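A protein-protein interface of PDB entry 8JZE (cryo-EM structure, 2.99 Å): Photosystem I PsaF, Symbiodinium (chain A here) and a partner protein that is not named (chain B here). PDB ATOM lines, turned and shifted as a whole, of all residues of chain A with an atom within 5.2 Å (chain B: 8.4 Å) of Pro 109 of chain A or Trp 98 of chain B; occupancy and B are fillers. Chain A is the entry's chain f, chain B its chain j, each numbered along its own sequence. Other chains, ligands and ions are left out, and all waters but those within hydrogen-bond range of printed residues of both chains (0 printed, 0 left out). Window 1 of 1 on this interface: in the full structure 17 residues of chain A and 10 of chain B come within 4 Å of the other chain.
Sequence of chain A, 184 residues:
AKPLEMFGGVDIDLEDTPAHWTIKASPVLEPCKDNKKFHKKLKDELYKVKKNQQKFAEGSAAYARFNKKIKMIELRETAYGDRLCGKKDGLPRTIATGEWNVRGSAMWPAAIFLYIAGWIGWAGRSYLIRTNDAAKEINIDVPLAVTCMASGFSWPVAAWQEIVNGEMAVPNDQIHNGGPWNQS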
ATOM      1  N   ARG A  83      -5.990 -21.102  -5.739  1.00  0.00           N
ATOM      2  CA  ARG A  83      -7.236 -20.397  -5.478  1.00  0.00           C
ATOM      3  C   ARG A  83      -7.485 -19.349  -6.559  1.00  0.00           C
ATOM      4  O   ARG A  83      -6.555 -18.739  -7.089  1.00  0.00           O
ATOM      5  CB  ARG A  83      -7.203 -19.746  -4.094  1.00  0.00           C
ATOM      6  CG  ARG A  83      -8.577 -19.523  -3.476  1.00  0.00           C
ATOM      7  CD  ARG A  83      -8.483 -19.055  -2.026  1.00  0.00           C
ATOM      8  NE  ARG A  83      -7.889 -20.058  -1.150  1.00  0.00           N
ATOM      9  CZ  ARG A  83      -7.677 -19.887   0.149  1.00  0.00           C
ATOM     10  NH1 ARG A  83      -7.992 -18.756   0.758  1.00  0.00           N
ATOM     11  NH2 ARG A  83      -7.134 -20.876   0.853  1.00  0.00           N
ATOM     12  N   THR A  94     -13.824 -16.671  -2.792  1.00  0.00           N
ATOM     13  CA  THR A  94     -14.492 -17.794  -2.153  1.00  0.00           C
ATOM     14  C   THR A  94     -15.658 -18.228  -3.030  1.00  0.00           C
ATOM     15  O   THR A  94     -16.466 -17.396  -3.453  1.00  0.00           O
ATOM     16  CB  THR A  94     -14.987 -17.420  -0.753  1.00  0.00           C
ATOM     17  OG1 THR A  94     -13.864 -17.229   0.118  1.00  0.00           O
ATOM     18  CG2 THR A  94     -15.879 -18.514  -0.188  1.00  0.00           C
ATOM     19  N   VAL A 102     -13.557 -27.220  -5.516  1.00  0.00           N
ATOM     20  CA  VAL A 102     -12.654 -26.140  -5.893  1.00  0.00           C
ATOM     21  C   VAL A 102     -11.982 -25.596  -4.642  1.00  0.00           C
ATOM     22  O   VAL A 102     -12.496 -25.714  -3.528  1.00  0.00           O
ATOM     23  CB  VAL A 102     -13.366 -24.994  -6.646  1.00  0.00           C
ATOM     24  CG1 VAL A 102     -13.693 -25.411  -8.064  1.00  0.00           C
ATOM     25  CG2 VAL A 102     -14.619 -24.575  -5.908  1.00  0.00           C
ATOM     26  N   ARG A 103     -10.814 -24.994  -4.843  1.00  0.00           N
ATOM     27  CA  ARG A 103     -10.109 -24.348  -3.748  1.00  0.00           C
ATOM     28  C   ARG A 103     -10.913 -23.154  -3.249  1.00  0.00           C
ATOM     29  O   ARG A 103     -11.417 -22.355  -4.043  1.00  0.00           O
ATOM     30  CB  ARG A 103      -8.721 -23.901  -4.206  1.00  0.00           C
ATOM     31  CG  ARG A 103      -7.773 -25.045  -4.528  1.00  0.00           C
ATOM     32  CD  ARG A 103      -7.378 -25.790  -3.269  1.00  0.00           C
ATOM     33  NE  ARG A 103      -6.984 -24.866  -2.212  1.00  0.00           N
ATOM     34  CZ  ARG A 103      -5.782 -24.318  -2.106  1.00  0.00           C
ATOM     35  NH1 ARG A 103      -4.818 -24.592  -2.969  1.00  0.00           N
ATOM     36  NH2 ARG A 103      -5.542 -23.470  -1.111  1.00  0.00           N
ATOM     37  N   GLY A 104     -11.037 -23.037  -1.930  1.00  0.00           N
ATOM     38  CA  GLY A 104     -11.786 -21.937  -1.361  1.00  0.00           C
ATOM     39  C   GLY A 104     -13.286 -22.059  -1.478  1.00  0.00           C
ATOM     40  O   GLY A 104     -13.988 -21.052  -1.365  1.00  0.00           O
ATOM     41  N   SER A 105     -13.801 -23.264  -1.707  1.00  0.00           N
ATOM     42  CA  SER A 105     -15.242 -23.460  -1.788  1.00  0.00           C
ATOM     43  C   SER A 105     -15.885 -23.301  -0.415  1.00  0.00           C
ATOM     44  O   SER A 105     -15.290 -23.620   0.617  1.00  0.00           O
ATOM     45  CB  SER A 105     -15.563 -24.841  -2.356  1.00  0.00           C
ATOM     46  OG  SER A 105     -16.959 -25.080  -2.344  1.00  0.00           O
ATOM     47  N   ALA A 106     -17.118 -22.803  -0.411  1.00  0.00           N
ATOM     48  CA  ALA A 106     -17.857 -22.575   0.822  1.00  0.00           C
ATOM     49  C   ALA A 106     -18.701 -23.768   1.242  1.00  0.00           C
ATOM     50  O   ALA A 106     -19.408 -23.681   2.249  1.00  0.00           O
ATOM     51  CB  ALA A 106     -18.752 -21.339   0.683  1.00  0.00           C
ATOM     52  N   MET A 107     -18.651 -24.875   0.499  1.00  0.00           N
ATOM     53  CA  MET A 107     -19.476 -26.031   0.836  1.00  0.00           C
ATOM     54  C   MET A 107     -18.952 -26.750   2.072  1.00  0.00           C
ATOM     55  O   MET A 107     -19.728 -27.129   2.955  1.00  0.00           O
ATOM     56  CB  MET A 107     -19.547 -26.990  -0.350  1.00  0.00           C
ATOM     57  CG  MET A 107     -20.546 -26.597  -1.419  1.00  0.00           C
ATOM     58  SD  MET A 107     -22.272 -26.900  -0.980  1.00  0.00           S
ATOM     59  CE  MET A 107     -22.743 -25.328  -0.265  1.00  0.00           C
ATOM     60  N   TRP A 108     -17.641 -26.971   2.139  1.00  0.00           N
ATOM     61  CA  TRP A 108     -17.071 -27.663   3.294  1.00  0.00           C
ATOM     62  C   TRP A 108     -17.235 -26.877   4.590  1.00  0.00           C
ATOM     63  O   TRP A 108     -17.669 -27.472   5.594  1.00  0.00           O
ATOM     64  CB  TRP A 108     -15.602 -27.999   3.012  1.00  0.00           C
ATOM     65  CG  TRP A 108     -15.417 -28.861   1.802  1.00  0.00           C
ATOM     66  CD1 TRP A 108     -15.139 -28.448   0.531  1.00  0.00           C
ATOM     67  CD2 TRP A 108     -15.509 -30.288   1.749  1.00  0.00           C
ATOM     68  NE1 TRP A 108     -15.048 -29.531  -0.309  1.00  0.00           N
ATOM     69  CE2 TRP A 108     -15.271 -30.673   0.416  1.00  0.00           C
ATOM     70  CE3 TRP A 108     -15.767 -31.277   2.701  1.00  0.00           C
ATOM     71  CZ2 TRP A 108     -15.284 -32.006   0.012  1.00  0.00           C
ATOM     72  CZ3 TRP A 108     -15.780 -32.598   2.300  1.00  0.00           C
ATOM     73  CH2 TRP A 108     -15.540 -32.951   0.967  1.00  0.00           C
ATOM     74  N   PRO A 109     -16.899 -25.580   4.659  1.00  0.00           N
ATOM     75  CA  PRO A 109     -17.177 -24.841   5.900  1.00  0.00           C
ATOM     76  C   PRO A 109     -18.652 -24.805   6.241  1.00  0.00           C
ATOM     77  O   PRO A 109     -19.010 -24.874   7.422  1.00  0.00           O
ATOM     78  CB  PRO A 109     -16.623 -23.439   5.607  1.00  0.00           C
ATOM     79  CG  PRO A 109     -15.647 -23.633   4.508  1.00  0.00           C
ATOM     80  CD  PRO A 109     -16.224 -24.723   3.668  1.00  0.00           C
ATOM     81  N   ALA A 110     -19.522 -24.711   5.232  1.00  0.00           N
ATOM     82  CA  ALA A 110     -20.957 -24.709   5.492  1.00  0.00           C
ATOM     83  C   ALA A 110     -21.396 -26.018   6.127  1.00  0.00           C
ATOM     84  O   ALA A 110     -22.148 -26.023   7.106  1.00  0.00           O
ATOM     85  CB  ALA A 110     -21.730 -24.457   4.197  1.00  0.00           C
ATOM     86  N   ALA A 111     -20.926 -27.143   5.585  1.00  0.00           N
ATOM     87  CA  ALA A 111     -21.302 -28.442   6.131  1.00  0.00           C
ATOM     88  C   ALA A 111     -20.795 -28.599   7.557  1.00  0.00           C
ATOM     89  O   ALA A 111     -21.542 -29.013   8.456  1.00  0.00           O
ATOM     90  CB  ALA A 111     -20.765 -29.561   5.238  1.00  0.00           C
ATOM     91  N   ILE A 112     -19.526 -28.250   7.789  1.00  0.00           N
ATOM     92  CA  ILE A 112     -18.956 -28.398   9.126  1.00  0.00           C
ATOM     93  C   ILE A 112     -19.716 -27.534  10.124  1.00  0.00           C
ATOM     94  O   ILE A 112     -20.120 -28.003  11.200  1.00  0.00           O
ATOM     95  CB  ILE A 112     -17.454 -28.060   9.116  1.00  0.00           C
ATOM     96  CG1 ILE A 112     -16.678 -29.079   8.280  1.00  0.00           C
ATOM     97  CG2 ILE A 112     -16.913 -28.025  10.534  1.00  0.00           C
ATOM     98  CD1 ILE A 112     -15.175 -28.883   8.320  1.00  0.00           C
ATOM     99  N   PHE A 113     -19.946 -26.261   9.776  1.00  0.00           N
ATOM    100  CA  PHE A 113     -20.636 -25.381  10.708  1.00  0.00           C
ATOM    101  C   PHE A 113     -22.061 -25.840  10.954  1.00  0.00           C
ATOM    102  O   PHE A 113     -22.547 -25.757  12.080  1.00  0.00           O
ATOM    103  CB  PHE A 113     -20.672 -23.934  10.230  1.00  0.00           C
ATOM    104  CG  PHE A 113     -21.506 -23.063  11.121  1.00  0.00           C
ATOM    105  CD1 PHE A 113     -20.962 -22.514  12.268  1.00  0.00           C
ATOM    106  CD2 PHE A 113     -22.853 -22.856  10.859  1.00  0.00           C
ATOM    107  CE1 PHE A 113     -21.728 -21.743  13.116  1.00  0.00           C
ATOM    108  CE2 PHE A 113     -23.625 -22.097  11.707  1.00  0.00           C
ATOM    109  CZ  PHE A 113     -23.062 -21.540  12.839  1.00  0.00           C
ATOM    110  N   LEU A 114     -22.773 -26.255   9.907  1.00  0.00           N
ATOM    111  CA  LEU A 114     -24.151 -26.672  10.111  1.00  0.00           C
ATOM    112  C   LEU A 114     -24.213 -27.879  11.030  1.00  0.00           C
ATOM    113  O   LEU A 114     -25.061 -27.938  11.929  1.00  0.00           O
ATOM    114  CB  LEU A 114     -24.826 -26.961   8.772  1.00  0.00           C
ATOM    115  CG  LEU A 114     -25.240 -25.704   8.003  1.00  0.00           C
ATOM    116  CD1 LEU A 114     -26.011 -26.064   6.749  1.00  0.00           C
ATOM    117  CD2 LEU A 114     -26.060 -24.788   8.893  1.00  0.00           C
ATOM    118  N   PRO B  93      -2.060 -21.771  10.791  1.00  0.00           N
ATOM    119  CA  PRO B  93      -2.297 -20.370  10.441  1.00  0.00           C
ATOM    120  C   PRO B  93      -2.577 -20.196   8.957  1.00  0.00           C
ATOM    121  O   PRO B  93      -2.188 -21.010   8.117  1.00  0.00           O
ATOM    122  CB  PRO B  93      -0.990 -19.682  10.842  1.00  0.00           C
ATOM    123  CG  PRO B  93       0.039 -20.739  10.655  1.00  0.00           C
ATOM    124  CD  PRO B  93      -0.628 -22.045  11.013  1.00  0.00           C
ATOM    125  N   ASP B  94      -3.278 -19.108   8.648  1.00  0.00           N
ATOM    126  CA  ASP B  94      -3.572 -18.654   7.291  1.00  0.00           C
ATOM    127  C   ASP B  94      -4.435 -19.634   6.501  1.00  0.00           C
ATOM    128  O   ASP B  94      -4.557 -19.484   5.278  1.00  0.00           O
ATOM    129  CB  ASP B  94      -2.285 -18.351   6.512  1.00  0.00           C
ATOM    130  CG  ASP B  94      -1.388 -17.361   7.228  1.00  0.00           C
ATOM    131  OD1 ASP B  94      -1.663 -17.048   8.406  1.00  0.00           O
ATOM    132  OD2 ASP B  94      -0.406 -16.893   6.613  1.00  0.00           O
ATOM    133  N   THR B  95      -5.043 -20.616   7.173  1.00  0.00           N
ATOM    134  CA  THR B  95      -5.921 -21.640   6.579  1.00  0.00           C
ATOM    135  C   THR B  95      -5.443 -22.069   5.190  1.00  0.00           C
ATOM    136  O   THR B  95      -6.185 -22.050   4.205  1.00  0.00           O
ATOM    137  CB  THR B  95      -7.391 -21.188   6.558  1.00  0.00           C
ATOM    138  OG1 THR B  95      -8.199 -22.207   5.954  1.00  0.00           O
ATOM    139  CG2 THR B  95      -7.597 -19.876   5.804  1.00  0.00           C
ATOM    140  N   LEU B  96      -4.173 -22.474   5.126  1.00  0.00           N
ATOM    141  CA  LEU B  96      -3.575 -22.870   3.854  1.00  0.00           C
ATOM    142  C   LEU B  96      -4.252 -24.104   3.271  1.00  0.00           C
ATOM    143  O   LEU B  96      -4.341 -24.243   2.046  1.00  0.00           O
ATOM    144  CB  LEU B  96      -2.078 -23.122   4.045  1.00  0.00           C
ATOM    145  CG  LEU B  96      -1.303 -22.012   4.758  1.00  0.00           C
ATOM    146  CD1 LEU B  96       0.139 -22.420   5.002  1.00  0.00           C
ATOM    147  CD2 LEU B  96      -1.365 -20.727   3.957  1.00  0.00           C
ATOM    148  N   TYR B  97      -4.741 -25.000   4.130  1.00  0.00           N
ATOM    149  CA  TYR B  97      -5.376 -26.233   3.680  1.00  0.00           C
ATOM    150  C   TYR B  97      -6.659 -25.989   2.896  1.00  0.00           C
ATOM    151  O   TYR B  97      -7.069 -26.861   2.122  1.00  0.00           O
ATOM    152  CB  TYR B  97      -5.677 -27.124   4.886  1.00  0.00           C
ATOM    153  CG  TYR B  97      -6.366 -26.385   6.010  1.00  0.00           C
ATOM    154  CD1 TYR B  97      -7.748 -26.253   6.035  1.00  0.00           C
ATOM    155  CD2 TYR B  97      -5.633 -25.813   7.041  1.00  0.00           C
ATOM    156  CE1 TYR B  97      -8.380 -25.575   7.057  1.00  0.00           C
ATOM    157  CE2 TYR B  97      -6.256 -25.133   8.065  1.00  0.00           C
ATOM    158  CZ  TYR B  97      -7.629 -25.018   8.068  1.00  0.00           C
ATOM    159  OH  TYR B  97      -8.253 -24.343   9.087  1.00  0.00           O
ATOM    160  N   TRP B  98      -7.301 -24.840   3.078  1.00  0.00           N
ATOM    161  CA  TRP B  98      -8.573 -24.560   2.419  1.00  0.00           C
ATOM    162  C   TRP B  98      -8.389 -24.380   0.917  1.00  0.00           C
ATOM    163  O   TRP B  98      -7.351 -23.903   0.461  1.00  0.00           O
ATOM    164  CB  TRP B  98      -9.231 -23.313   3.014  1.00  0.00           C
ATOM    165  CG  TRP B  98     -10.659 -23.140   2.591  1.00  0.00           C
ATOM    166  CD1 TRP B  98     -11.521 -24.122   2.200  1.00  0.00           C
ATOM    167  CD2 TRP B  98     -11.389 -21.909   2.504  1.00  0.00           C
ATOM    168  NE1 TRP B  98     -12.743 -23.580   1.881  1.00  0.00           N
ATOM    169  CE2 TRP B  98     -12.687 -22.223   2.059  1.00  0.00           C
ATOM    170  CE3 TRP B  98     -11.070 -20.572   2.762  1.00  0.00           C
ATOM    171  CZ2 TRP B  98     -13.666 -21.250   1.866  1.00  0.00           C
ATOM    172  CZ3 TRP B  98     -12.044 -19.608   2.569  1.00  0.00           C
ATOM    173  CH2 TRP B  98     -13.324 -19.952   2.125  1.00  0.00           C
ATOM    174  OXT TRP B  98      -9.274 -24.707   0.127  1.00  0.00           O
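The guanidinium group (NH2) of Arg 83 of chain A lies within salt-bridge range of the chain-end carboxylate (O) of Trp 98 of chain B (3.1 Å). The guanidinium group (NH2) of Arg 103 of chain A lies within hydrogen-bond range of the backbone carbonyl oxygen (O) of Leu 96 of chain B, at 3.5 Å. The guanidinium group (NH2) of Arg 103 of chain A lies within salt-bridge range of the chain-end carboxylate (O) of Trp 98 of chain B (2.4 Å). The chain-end carboxylate of Trp 98 of chain B sits at hydrogen-bond distance from the backbone NH of Gly 104 of chain A (3.2 Å). The backbone carbonyl oxygen of Ser 105 of chain A is in hydrogen-bond range of the indole nitrogen of Trp 98 of chain B (2.8 Å).
The side-chain hydroxyl of Ser 105 of chain A sits close to the backbone NH of Met 107 of chain A (3.3 Å).
Arg 83 of chain A touches Thr 95 of chain B (NH2 to O, 3.7 Å). Thr 94 of chain A touches Trp 98 of chain B. Trp 98 of chain B touches Pro 109 of chain A.
Printed residues of chain A within 4 Å of Trp 98 of chain B: Arg 83 (3.1 Å), Thr 94 (3.4 Å), Arg 103 (2.4 Å), Gly 104 (3.2 Å), Ser 105 (2.8 Å) and Pro 109 (3.9 Å). Printed residues of chain B within 4 Å of Ser 105 of chain A: Trp 98 (2.8 Å). Of the printed residues of chain B, Arg 103 of chain A touches Leu 96 and Trp 98. Of the printed residues of chain A, Leu 96 of chain B touches Arg 103 (3.5 Å). Of the printed residues of chain B, Arg 83 of chain A touches Thr 95 and Trp 98. Ala 111 of chain A touches none of the printed residues of chain B. Pro 93 of chain B touches none of the printed residues of chain A.
Hydrophobic or aromatic side chains of chain B that line the printed part of chain A: Trp 98. Among the printed residues, no Asp or Glu carboxylate lies within 4 Å of a Lys or Arg side-chain nitrogen of the other chain.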
